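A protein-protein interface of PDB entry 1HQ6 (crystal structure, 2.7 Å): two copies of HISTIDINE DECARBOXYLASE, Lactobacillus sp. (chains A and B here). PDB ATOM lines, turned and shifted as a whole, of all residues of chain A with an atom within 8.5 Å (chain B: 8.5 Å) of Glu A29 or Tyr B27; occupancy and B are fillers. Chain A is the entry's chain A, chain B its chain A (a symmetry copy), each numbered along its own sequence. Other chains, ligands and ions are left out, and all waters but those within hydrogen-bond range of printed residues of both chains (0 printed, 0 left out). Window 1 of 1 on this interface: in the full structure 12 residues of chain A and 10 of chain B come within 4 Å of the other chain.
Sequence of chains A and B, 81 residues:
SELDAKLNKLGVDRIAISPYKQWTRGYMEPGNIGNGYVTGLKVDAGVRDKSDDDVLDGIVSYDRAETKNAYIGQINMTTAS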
ATOM      1  N   ILE A  17      30.801 -17.756   9.421  1.00  0.00           N
ATOM      2  CA  ILE A  17      31.981 -18.549   9.703  1.00  0.00           C
ATOM      3  C   ILE A  17      31.672 -19.405  10.923  1.00  0.00           C
ATOM      4  O   ILE A  17      30.957 -18.970  11.822  1.00  0.00           O
ATOM      5  CB  ILE A  17      33.190 -17.579   9.943  1.00  0.00           C
ATOM      6  CG1 ILE A  17      33.979 -17.405   8.668  1.00  0.00           C
ATOM      7  CG2 ILE A  17      34.186 -18.143  10.940  1.00  0.00           C
ATOM      8  CD1 ILE A  17      33.431 -16.431   7.632  1.00  0.00           C
ATOM      9  N   SER A  18      32.220 -20.602  10.992  1.00  0.00           N
ATOM     10  CA  SER A  18      32.016 -21.533  12.086  1.00  0.00           C
ATOM     11  C   SER A  18      33.317 -21.489  12.850  1.00  0.00           C
ATOM     12  O   SER A  18      34.380 -21.496  12.239  1.00  0.00           O
ATOM     13  CB  SER A  18      31.772 -22.945  11.551  1.00  0.00           C
ATOM     14  OG  SER A  18      32.229 -24.014  12.380  1.00  0.00           O
ATOM     15  N   PRO A  19      33.336 -21.441  14.163  1.00  0.00           N
ATOM     16  CA  PRO A  19      34.553 -21.528  14.930  1.00  0.00           C
ATOM     17  C   PRO A  19      35.165 -22.903  15.004  1.00  0.00           C
ATOM     18  O   PRO A  19      36.297 -23.001  15.459  1.00  0.00           O
ATOM     19  CB  PRO A  19      34.165 -20.998  16.268  1.00  0.00           C
ATOM     20  CG  PRO A  19      32.697 -21.281  16.379  1.00  0.00           C
ATOM     21  CD  PRO A  19      32.235 -20.965  14.977  1.00  0.00           C
ATOM     22  N   TYR A  20      34.477 -23.970  14.575  1.00  0.00           N
ATOM     23  CA  TYR A  20      34.984 -25.325  14.773  1.00  0.00           C
ATOM     24  C   TYR A  20      36.001 -25.811  13.781  1.00  0.00           C
ATOM     25  O   TYR A  20      36.106 -25.341  12.648  1.00  0.00           O
ATOM     26  CB  TYR A  20      33.843 -26.322  14.755  1.00  0.00           C
ATOM     27  CG  TYR A  20      32.808 -26.183  15.851  1.00  0.00           C
ATOM     28  CD1 TYR A  20      32.953 -25.220  16.828  1.00  0.00           C
ATOM     29  CD2 TYR A  20      31.712 -27.043  15.879  1.00  0.00           C
ATOM     30  CE1 TYR A  20      32.026 -25.094  17.838  1.00  0.00           C
ATOM     31  CE2 TYR A  20      30.764 -26.926  16.899  1.00  0.00           C
ATOM     32  CZ  TYR A  20      30.939 -25.940  17.870  1.00  0.00           C
ATOM     33  OH  TYR A  20      30.041 -25.796  18.901  1.00  0.00           O
ATOM     34  N   TRP A  23      34.033 -29.094  11.088  1.00  0.00           N
ATOM     35  CA  TRP A  23      32.599 -28.993  11.101  1.00  0.00           C
ATOM     36  C   TRP A  23      31.923 -27.694  10.765  1.00  0.00           C
ATOM     37  O   TRP A  23      32.390 -26.612  11.117  1.00  0.00           O
ATOM     38  CB  TRP A  23      32.111 -29.398  12.458  1.00  0.00           C
ATOM     39  CG  TRP A  23      32.497 -30.789  12.932  1.00  0.00           C
ATOM     40  CD1 TRP A  23      32.452 -31.879  12.109  1.00  0.00           C
ATOM     41  CD2 TRP A  23      32.871 -31.102  14.219  1.00  0.00           C
ATOM     42  NE1 TRP A  23      32.778 -32.874  12.885  1.00  0.00           N
ATOM     43  CE2 TRP A  23      33.034 -32.474  14.127  1.00  0.00           C
ATOM     44  CE3 TRP A  23      33.088 -30.470  15.439  1.00  0.00           C
ATOM     45  CZ2 TRP A  23      33.414 -33.227  15.225  1.00  0.00           C
ATOM     46  CZ3 TRP A  23      33.470 -31.222  16.547  1.00  0.00           C
ATOM     47  CH2 TRP A  23      33.624 -32.596  16.446  1.00  0.00           C
ATOM     48  N   THR A  24      30.799 -27.766  10.071  1.00  0.00           N
ATOM     49  CA  THR A  24      29.953 -26.603   9.841  1.00  0.00           C
ATOM     50  C   THR A  24      29.037 -26.580  11.041  1.00  0.00           C
ATOM     51  O   THR A  24      28.837 -27.591  11.738  1.00  0.00           O
ATOM     52  CB  THR A  24      29.068 -26.741   8.611  1.00  0.00           C
ATOM     53  OG1 THR A  24      28.721 -28.124   8.532  1.00  0.00           O
ATOM     54  CG2 THR A  24      29.731 -26.329   7.339  1.00  0.00           C
ATOM     55  N   ARG A  25      28.454 -25.428  11.282  1.00  0.00           N
ATOM     56  CA  ARG A  25      27.454 -25.255  12.318  1.00  0.00           C
ATOM     57  C   ARG A  25      26.241 -24.644  11.646  1.00  0.00           C
ATOM     58  O   ARG A  25      26.270 -24.343  10.449  1.00  0.00           O
ATOM     59  CB  ARG A  25      27.958 -24.323  13.391  1.00  0.00           C
ATOM     60  CG  ARG A  25      29.074 -24.925  14.193  1.00  0.00           C
ATOM     61  CD  ARG A  25      29.530 -23.848  15.133  1.00  0.00           C
ATOM     62  NE  ARG A  25      28.937 -23.953  16.443  1.00  0.00           N
ATOM     63  CZ  ARG A  25      28.671 -22.865  17.164  1.00  0.00           C
ATOM     64  NH1 ARG A  25      28.139 -23.022  18.362  1.00  0.00           N
ATOM     65  NH2 ARG A  25      28.888 -21.628  16.708  1.00  0.00           N
ATOM     66  N   GLY A  26      25.160 -24.430  12.385  1.00  0.00           N
ATOM     67  CA  GLY A  26      23.940 -23.917  11.803  1.00  0.00           C
ATOM     68  C   GLY A  26      23.749 -22.459  12.102  1.00  0.00           C
ATOM     69  O   GLY A  26      24.324 -21.902  13.047  1.00  0.00           O
ATOM     70  N   TYR A  27      22.955 -21.835  11.253  1.00  0.00           N
ATOM     71  CA  TYR A  27      22.624 -20.442  11.386  1.00  0.00           C
ATOM     72  C   TYR A  27      21.978 -20.222  12.734  1.00  0.00           C
ATOM     73  O   TYR A  27      21.223 -21.064  13.185  1.00  0.00           O
ATOM     74  CB  TYR A  27      21.701 -20.085  10.247  1.00  0.00           C
ATOM     75  CG  TYR A  27      21.166 -18.678  10.248  1.00  0.00           C
ATOM     76  CD1 TYR A  27      22.033 -17.595  10.219  1.00  0.00           C
ATOM     77  CD2 TYR A  27      19.792 -18.475  10.300  1.00  0.00           C
ATOM     78  CE1 TYR A  27      21.522 -16.301  10.253  1.00  0.00           C
ATOM     79  CE2 TYR A  27      19.269 -17.177  10.334  1.00  0.00           C
ATOM     80  CZ  TYR A  27      20.150 -16.111  10.313  1.00  0.00           C
ATOM     81  OH  TYR A  27      19.657 -14.850  10.386  1.00  0.00           O
ATOM     82  N   MET A  28      22.321 -19.091  13.355  1.00  0.00           N
ATOM     83  CA  MET A  28      21.898 -18.626  14.668  1.00  0.00           C
ATOM     84  C   MET A  28      22.539 -19.307  15.867  1.00  0.00           C
ATOM     85  O   MET A  28      22.246 -18.944  17.010  1.00  0.00           O
ATOM     86  CB  MET A  28      20.352 -18.699  14.811  1.00  0.00           C
ATOM     87  CG  MET A  28      19.613 -17.651  13.972  1.00  0.00           C
ATOM     88  SD  MET A  28      17.800 -17.662  14.076  1.00  0.00           S
ATOM     89  CE  MET A  28      17.519 -19.234  13.324  1.00  0.00           C
ATOM     90  N   GLU A  29      23.473 -20.238  15.677  1.00  0.00           N
ATOM     91  CA  GLU A  29      24.190 -20.869  16.787  1.00  0.00           C
ATOM     92  C   GLU A  29      25.261 -19.983  17.415  1.00  0.00           C
ATOM     93  O   GLU A  29      26.000 -19.319  16.679  1.00  0.00           O
ATOM     94  CB  GLU A  29      24.869 -22.139  16.341  1.00  0.00           C
ATOM     95  CG  GLU A  29      23.851 -23.220  16.081  1.00  0.00           C
ATOM     96  CD  GLU A  29      24.380 -24.638  16.100  1.00  0.00           C
ATOM     97  OE1 GLU A  29      25.207 -25.017  15.276  1.00  0.00           O
ATOM     98  OE2 GLU A  29      23.949 -25.379  16.973  1.00  0.00           O
ATOM     99  N   PRO A  30      25.431 -19.924  18.744  1.00  0.00           N
ATOM    100  CA  PRO A  30      26.295 -18.976  19.416  1.00  0.00           C
ATOM    101  C   PRO A  30      27.758 -19.239  19.136  1.00  0.00           C
ATOM    102  O   PRO A  30      28.222 -20.377  19.179  1.00  0.00           O
ATOM    103  CB  PRO A  30      25.911 -19.120  20.866  1.00  0.00           C
ATOM    104  CG  PRO A  30      25.563 -20.560  20.996  1.00  0.00           C
ATOM    105  CD  PRO A  30      24.796 -20.795  19.712  1.00  0.00           C
ATOM    106  N   GLY A  31      28.508 -18.191  18.829  1.00  0.00           N
ATOM    107  CA  GLY A  31      29.922 -18.332  18.589  1.00  0.00           C
ATOM    108  C   GLY A  31      30.214 -18.253  17.122  1.00  0.00           C
ATOM    109  O   GLY A  31      31.380 -18.228  16.737  1.00  0.00           O
ATOM    110  N   ASN A  32      29.213 -18.218  16.253  1.00  0.00           N
ATOM    111  CA  ASN A  32      29.478 -18.104  14.823  1.00  0.00           C
ATOM    112  C   ASN A  32      29.913 -16.688  14.546  1.00  0.00           C
ATOM    113  O   ASN A  32      29.551 -15.766  15.275  1.00  0.00           O
ATOM    114  CB  ASN A  32      28.249 -18.375  13.964  1.00  0.00           C
ATOM    115  CG  ASN A  32      27.848 -19.834  13.755  1.00  0.00           C
ATOM    116  OD1 ASN A  32      28.670 -20.740  13.693  1.00  0.00           O
ATOM    117  ND2 ASN A  32      26.575 -20.128  13.547  1.00  0.00           N
ATOM    118  N   ILE A  33      30.711 -16.463  13.518  1.00  0.00           N
ATOM    119  CA  ILE A  33      31.108 -15.107  13.200  1.00  0.00           C
ATOM    120  C   ILE A  33      30.355 -14.728  11.950  1.00  0.00           C
ATOM    121  O   ILE A  33      30.351 -15.459  10.961  1.00  0.00           O
ATOM    122  CB  ILE A  33      32.616 -15.025  12.983  1.00  0.00           C
ATOM    123  CG1 ILE A  33      33.296 -15.386  14.293  1.00  0.00           C
ATOM    124  CG2 ILE A  33      33.019 -13.633  12.514  1.00  0.00           C
ATOM    125  CD1 ILE A  33      34.781 -15.005  14.431  1.00  0.00           C
ATOM    126  N   GLY A  34      29.671 -13.608  12.026  1.00  0.00           N
ATOM    127  CA  GLY A  34      28.923 -13.135  10.893  1.00  0.00           C
ATOM    128  C   GLY A  34      27.427 -13.206  11.075  1.00  0.00           C
ATOM    129  O   GLY A  34      26.881 -13.901  11.920  1.00  0.00           O
ATOM    130  N   GLY A  36      25.124 -13.958   8.533  1.00  0.00           N
ATOM    131  CA  GLY A  36      24.572 -14.523   7.323  1.00  0.00           C
ATOM    132  C   GLY A  36      24.524 -16.040   7.391  1.00  0.00           C
ATOM    133  O   GLY A  36      24.808 -16.671   8.419  1.00  0.00           O
ATOM    134  N   ILE A  75      22.559 -34.659  13.492  1.00  0.00           N
ATOM    135  CA  ILE A  75      22.146 -33.279  13.560  1.00  0.00           C
ATOM    136  C   ILE A  75      20.755 -33.112  14.137  1.00  0.00           C
ATOM    137  O   ILE A  75      19.937 -34.018  14.055  1.00  0.00           O
ATOM    138  CB  ILE A  75      22.320 -32.794  12.101  1.00  0.00           C
ATOM    139  CG1 ILE A  75      23.325 -31.698  12.238  1.00  0.00           C
ATOM    140  CG2 ILE A  75      21.067 -32.343  11.364  1.00  0.00           C
ATOM    141  CD1 ILE A  75      24.699 -32.188  12.716  1.00  0.00           C
ATOM    142  N   ASN A  76      20.471 -31.978  14.752  1.00  0.00           N
ATOM    143  CA  ASN A  76      19.154 -31.725  15.283  1.00  0.00           C
ATOM    144  C   ASN A  76      18.622 -30.761  14.280  1.00  0.00           C
ATOM    145  O   ASN A  76      19.274 -29.727  14.089  1.00  0.00           O
ATOM    146  CB  ASN A  76      19.172 -31.004  16.574  1.00  0.00           C
ATOM    147  CG  ASN A  76      19.676 -31.814  17.724  1.00  0.00           C
ATOM    148  OD1 ASN A  76      18.933 -32.558  18.341  1.00  0.00           O
ATOM    149  ND2 ASN A  76      20.933 -31.720  18.073  1.00  0.00           N
ATOM    150  N   ASP B  13      33.192 -25.560  22.967  1.00  0.00           N
ATOM    151  CA  ASP B  13      33.151 -25.364  24.404  1.00  0.00           C
ATOM    152  C   ASP B  13      31.747 -25.741  24.864  1.00  0.00           C
ATOM    153  O   ASP B  13      30.786 -25.512  24.142  1.00  0.00           O
ATOM    154  CB  ASP B  13      33.409 -23.906  24.783  1.00  0.00           C
ATOM    155  CG  ASP B  13      32.398 -22.858  24.315  1.00  0.00           C
ATOM    156  OD1 ASP B  13      31.446 -22.606  25.051  1.00  0.00           O
ATOM    157  OD2 ASP B  13      32.580 -22.290  23.235  1.00  0.00           O
ATOM    158  N   ILE B  15      30.061 -24.329  27.415  1.00  0.00           N
ATOM    159  CA  ILE B  15      29.632 -23.356  28.428  1.00  0.00           C
ATOM    160  C   ILE B  15      28.250 -22.867  28.045  1.00  0.00           C
ATOM    161  O   ILE B  15      28.011 -22.598  26.869  1.00  0.00           O
ATOM    162  CB  ILE B  15      30.603 -22.166  28.486  1.00  0.00           C
ATOM    163  CG1 ILE B  15      32.007 -22.657  28.681  1.00  0.00           C
ATOM    164  CG2 ILE B  15      30.261 -21.268  29.639  1.00  0.00           C
ATOM    165  CD1 ILE B  15      33.068 -21.670  28.180  1.00  0.00           C
ATOM    166  N   ALA B  16      27.363 -22.733  29.020  1.00  0.00           N
ATOM    167  CA  ALA B  16      26.002 -22.289  28.800  1.00  0.00           C
ATOM    168  C   ALA B  16      25.511 -21.641  30.067  1.00  0.00           C
ATOM    169  O   ALA B  16      25.019 -22.310  30.971  1.00  0.00           O
ATOM    170  CB  ALA B  16      25.068 -23.445  28.513  1.00  0.00           C
ATOM    171  N   ILE B  17      25.629 -20.334  30.173  1.00  0.00           N
ATOM    172  CA  ILE B  17      25.237 -19.590  31.354  1.00  0.00           C
ATOM    173  C   ILE B  17      24.065 -18.701  30.965  1.00  0.00           C
ATOM    174  O   ILE B  17      24.009 -18.205  29.842  1.00  0.00           O
ATOM    175  CB  ILE B  17      26.473 -18.766  31.860  1.00  0.00           C
ATOM    176  CG1 ILE B  17      27.197 -19.525  32.944  1.00  0.00           C
ATOM    177  CG2 ILE B  17      26.058 -17.459  32.513  1.00  0.00           C
ATOM    178  CD1 ILE B  17      28.145 -20.637  32.509  1.00  0.00           C
ATOM    179  N   THR B  24      16.350 -20.359  33.985  1.00  0.00           N
ATOM    180  CA  THR B  24      17.180 -20.880  32.907  1.00  0.00           C
ATOM    181  C   THR B  24      16.609 -20.234  31.667  1.00  0.00           C
ATOM    182  O   THR B  24      15.456 -19.767  31.637  1.00  0.00           O
ATOM    183  CB  THR B  24      17.045 -22.385  32.724  1.00  0.00           C
ATOM    184  OG1 THR B  24      15.686 -22.697  33.032  1.00  0.00           O
ATOM    185  CG2 THR B  24      17.943 -23.184  33.607  1.00  0.00           C
ATOM    186  N   ARG B  25      17.406 -20.217  30.624  1.00  0.00           N
ATOM    187  CA  ARG B  25      16.983 -19.746  29.319  1.00  0.00           C
ATOM    188  C   ARG B  25      17.289 -20.860  28.339  1.00  0.00           C
ATOM    189  O   ARG B  25      17.855 -21.890  28.716  1.00  0.00           O
ATOM    190  CB  ARG B  25      17.749 -18.507  28.929  1.00  0.00           C
ATOM    191  CG  ARG B  25      17.387 -17.321  29.774  1.00  0.00           C
ATOM    192  CD  ARG B  25      18.301 -16.214  29.338  1.00  0.00           C
ATOM    193  NE  ARG B  25      17.697 -15.330  28.372  1.00  0.00           N
ATOM    194  CZ  ARG B  25      18.429 -14.746  27.425  1.00  0.00           C
ATOM    195  NH1 ARG B  25      17.825 -13.936  26.575  1.00  0.00           N
ATOM    196  NH2 ARG B  25      19.738 -14.977  27.282  1.00  0.00           N
ATOM    197  N   GLY B  26      16.946 -20.687  27.070  1.00  0.00           N
ATOM    198  CA  GLY B  26      17.139 -21.730  26.088  1.00  0.00           C
ATOM    199  C   GLY B  26      18.333 -21.465  25.219  1.00  0.00           C
ATOM    200  O   GLY B  26      18.812 -20.329  25.091  1.00  0.00           O
ATOM    201  N   TYR B  27      18.835 -22.544  24.649  1.00  0.00           N
ATOM    202  CA  TYR B  27      19.962 -22.494  23.758  1.00  0.00           C
ATOM    203  C   TYR B  27      19.628 -21.581  22.602  1.00  0.00           C
ATOM    204  O   TYR B  27      18.500 -21.576  22.144  1.00  0.00           O
ATOM    205  CB  TYR B  27      20.245 -23.905  23.305  1.00  0.00           C
ATOM    206  CG  TYR B  27      21.347 -24.064  22.293  1.00  0.00           C
ATOM    207  CD1 TYR B  27      22.633 -23.629  22.577  1.00  0.00           C
ATOM    208  CD2 TYR B  27      21.057 -24.636  21.059  1.00  0.00           C
ATOM    209  CE1 TYR B  27      23.632 -23.755  21.617  1.00  0.00           C
ATOM    210  CE2 TYR B  27      22.055 -24.766  20.087  1.00  0.00           C
ATOM    211  CZ  TYR B  27      23.329 -24.318  20.387  1.00  0.00           C
ATOM    212  OH  TYR B  27      24.295 -24.403  19.439  1.00  0.00           O
ATOM    213  N   MET B  28      20.627 -20.804  22.177  1.00  0.00           N
ATOM    214  CA  MET B  28      20.600 -19.806  21.119  1.00  0.00           C
ATOM    215  C   MET B  28      19.913 -18.490  21.447  1.00  0.00           C
ATOM    216  O   MET B  28      19.876 -17.588  20.605  1.00  0.00           O
ATOM    217  CB  MET B  28      19.978 -20.391  19.819  1.00  0.00           C
ATOM    218  CG  MET B  28      20.883 -21.411  19.119  1.00  0.00           C
ATOM    219  SD  MET B  28      20.237 -22.149  17.591  1.00  0.00           S
ATOM    220  CE  MET B  28      18.887 -23.038  18.297  1.00  0.00           C
ATOM    221  N   GLU B  29      19.423 -18.287  22.671  1.00  0.00           N
ATOM    222  CA  GLU B  29      18.828 -17.012  23.076  1.00  0.00           C
ATOM    223  C   GLU B  29      19.849 -15.911  23.347  1.00  0.00           C
ATOM    224  O   GLU B  29      20.877 -16.186  23.977  1.00  0.00           O
ATOM    225  CB  GLU B  29      18.004 -17.173  24.328  1.00  0.00           C
ATOM    226  CG  GLU B  29      16.737 -17.935  24.033  1.00  0.00           C
ATOM    227  CD  GLU B  29      15.618 -17.761  25.038  1.00  0.00           C
ATOM    228  OE1 GLU B  29      15.745 -18.136  26.200  1.00  0.00           O
ATOM    229  OE2 GLU B  29      14.592 -17.228  24.638  1.00  0.00           O
ATOM    230  N   PRO B  30      19.647 -14.651  22.935  1.00  0.00           N
ATOM    231  CA  PRO B  30      20.644 -13.602  22.994  1.00  0.00           C
ATOM    232  C   PRO B  30      20.963 -13.197  24.416  1.00  0.00           C
ATOM    233  O   PRO B  30      20.072 -13.015  25.244  1.00  0.00           O
ATOM    234  CB  PRO B  30      20.042 -12.501  22.162  1.00  0.00           C
ATOM    235  CG  PRO B  30      18.581 -12.631  22.408  1.00  0.00           C
ATOM    236  CD  PRO B  30      18.412 -14.135  22.383  1.00  0.00           C
ATOM    237  N   ASN B  32      23.063 -15.028  26.343  1.00  0.00           N
ATOM    238  CA  ASN B  32      23.594 -16.168  27.082  1.00  0.00           C
ATOM    239  C   ASN B  32      25.095 -16.129  26.974  1.00  0.00           C
ATOM    240  O   ASN B  32      25.643 -15.592  26.012  1.00  0.00           O
ATOM    241  CB  ASN B  32      23.134 -17.509  26.522  1.00  0.00           C
ATOM    242  CG  ASN B  32      21.718 -17.965  26.868  1.00  0.00           C
ATOM    243  OD1 ASN B  32      21.184 -17.698  27.938  1.00  0.00           O
ATOM    244  ND2 ASN B  32      21.070 -18.750  26.023  1.00  0.00           N
ATOM    245  N   GLY B  34      28.415 -18.291  26.523  1.00  0.00           N
ATOM    246  CA  GLY B  34      28.862 -19.609  26.165  1.00  0.00           C
ATOM    247  C   GLY B  34      28.250 -20.136  24.890  1.00  0.00           C
ATOM    248  O   GLY B  34      27.233 -19.679  24.388  1.00  0.00           O
ATOM    249  N   ASN B  35      28.876 -21.173  24.378  1.00  0.00           N
ATOM    250  CA  ASN B  35      28.487 -21.709  23.094  1.00  0.00           C
ATOM    251  C   ASN B  35      28.099 -23.162  23.246  1.00  0.00           C
ATOM    252  O   ASN B  35      28.443 -24.014  22.434  1.00  0.00           O
ATOM    253  CB  ASN B  35      29.635 -21.580  22.118  1.00  0.00           C
ATOM    254  CG  ASN B  35      30.176 -20.166  21.919  1.00  0.00           C
ATOM    255  OD1 ASN B  35      29.559 -19.137  22.187  1.00  0.00           O
ATOM    256  ND2 ASN B  35      31.399 -20.043  21.422  1.00  0.00           N
ATOM    257  N   GLY B  36      27.388 -23.491  24.310  1.00  0.00           N
ATOM    258  CA  GLY B  36      26.971 -24.851  24.567  1.00  0.00           C
ATOM    259  C   GLY B  36      25.556 -24.904  25.117  1.00  0.00           C
ATOM    260  O   GLY B  36      24.834 -23.899  25.198  1.00  0.00           O
ATOM    261  N   TYR B  37      25.137 -26.096  25.508  1.00  0.00           N
ATOM    262  CA  TYR B  37      23.786 -26.284  25.952  1.00  0.00           C
ATOM    263  C   TYR B  37      23.741 -27.370  26.992  1.00  0.00           C
ATOM    264  O   TYR B  37      24.621 -28.232  27.052  1.00  0.00           O
ATOM    265  CB  TYR B  37      22.915 -26.625  24.759  1.00  0.00           C
ATOM    266  CG  TYR B  37      23.341 -27.736  23.827  1.00  0.00           C
ATOM    267  CD1 TYR B  37      23.354 -29.048  24.274  1.00  0.00           C
ATOM    268  CD2 TYR B  37      23.650 -27.456  22.500  1.00  0.00           C
ATOM    269  CE1 TYR B  37      23.672 -30.093  23.415  1.00  0.00           C
ATOM    270  CE2 TYR B  37      23.964 -28.505  21.626  1.00  0.00           C
ATOM    271  CZ  TYR B  37      23.974 -29.817  22.097  1.00  0.00           C
ATOM    272  OH  TYR B  37      24.242 -30.863  21.267  1.00  0.00           O
ATOM    273  N   VAL B  38      22.743 -27.359  27.847  1.00  0.00           N
ATOM    274  CA  VAL B  38      22.609 -28.380  28.849  1.00  0.00           C
ATOM    275  C   VAL B  38      21.216 -28.956  28.643  1.00  0.00           C
ATOM    276  O   VAL B  38      20.268 -28.217  28.383  1.00  0.00           O
ATOM    277  CB  VAL B  38      22.804 -27.710  30.186  1.00  0.00           C
ATOM    278  CG1 VAL B  38      22.503 -28.639  31.333  1.00  0.00           C
ATOM    279  CG2 VAL B  38      24.244 -27.358  30.313  1.00  0.00           C
ATOM    280  N   THR B  39      21.074 -30.267  28.693  1.00  0.00           N
ATOM    281  CA  THR B  39      19.798 -30.880  28.437  1.00  0.00           C
ATOM    282  C   THR B  39      19.442 -31.819  29.580  1.00  0.00           C
ATOM    283  O   THR B  39      20.275 -32.190  30.417  1.00  0.00           O
ATOM    284  CB  THR B  39      19.922 -31.570  27.076  1.00  0.00           C
ATOM    285  OG1 THR B  39      18.638 -32.055  26.770  1.00  0.00           O
ATOM    286  CG2 THR B  39      20.931 -32.678  27.039  1.00  0.00           C
ATOM    287  N   THR B  78      10.243 -24.957  20.509  1.00  0.00           N
ATOM    288  CA  THR B  78      10.369 -25.141  19.078  1.00  0.00           C
ATOM    289  C   THR B  78      10.882 -26.562  18.982  1.00  0.00           C
ATOM    290  O   THR B  78      11.618 -27.016  19.861  1.00  0.00           O
ATOM    291  CB  THR B  78      11.365 -24.128  18.497  1.00  0.00           C
ATOM    292  OG1 THR B  78      12.405 -23.948  19.453  1.00  0.00           O
ATOM    293  CG2 THR B  78      10.741 -22.773  18.253  1.00  0.00           C
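The side-chain carboxylate (OE2) of Glu A29 sits at hydrogen-bond distance from the side-chain hydroxyl (OH) of Tyr B27, 2.7 Å away.
NH1 of Arg A25 sits at hydrogen-bond distance from O of Pro A30 (2.8 Å). O of Ile B15 is in hydrogen-bond range of N of Asn B35. ND2 of Asn A32 lies within hydrogen-bond range of O of Glu A29, 3.3 Å away. The backbone NH of Gly A26 sits at hydrogen-bond distance from the side-chain carboxylate of Glu A29. The backbone NH (N) of Asn B35 lies within hydrogen-bond range of the side-chain carboxylate (OD1) of Asp B13 (3.0 Å).
Met A28 touches Met B28 (O to CG, 3.5 Å). Tyr B27 touches Pro A30. Gly B34 touches Pro A30. Pro A30 touches Asn B35 (O to CG, 3.4 Å). Asn B35 touches Gly A31.
Printed residues of chain B within 4 Å of Glu A29: Tyr B27. Of chain A, only Glu A29 (2.7 Å) and Pro A30 (3.7 Å) come within 4 Å of Tyr B27. No residue of chain A comes within 4 Å of Gly B26. Of the printed residues of chain A, Asn B35 touches Pro A30 (3.4 Å) and Gly A31 (3.6 Å). Of the printed residues of chain A, Gly B34 touches Pro A30. Of the printed residues of chain A, Met B28 touches Met A28. Glu B29 touches none of the printed residues of chain A. The nearest residue of chain A that does not touch Tyr B27 is Arg A25 (4.2 Å). The nearest printed residue of chain A that does not touch Asn B35 is Arg A25 (4.2 Å).
Hydrophobic or aromatic side chains of chain B that line the printed part of chain A: Tyr B27 and Met B28. Of the 19 printed residues of chain A, 4 touch a printed residue of chain B. Printed residues of chain A that touch a printed residue of chain B: Met A28, Glu A29, Pro A30 and Gly A31. Hydrophobic or aromatic side chains of chain A that line the printed part of chain B: Pro A30. Among the printed residues, no Asp or Glu carboxylate lies within 4 Å of a Lys or Arg side-chain nitrogen of the other chain.
Met B28 touches its own counterpart, Met A28. Glu A29 touches Tyr B27, but with the chains exchanged Tyr A27 does not touch Glu B29 (10.0 Å). Pro A30 touches Tyr B27, but with the chains exchanged Tyr A27 does not touch Pro B30 (11.8 Å). Pro A30 touches Gly B34, but with the chains exchanged Gly A34 does not touch Pro B30 (12.4 Å). Positions printed for both chains: 17, 24, 25, 26, 27, 28, 29, 30, 32, 34 and 36. Of the 6 pairs that touch across the chains among the printed residues, 1 has its exchanged pair printed and touching as well.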
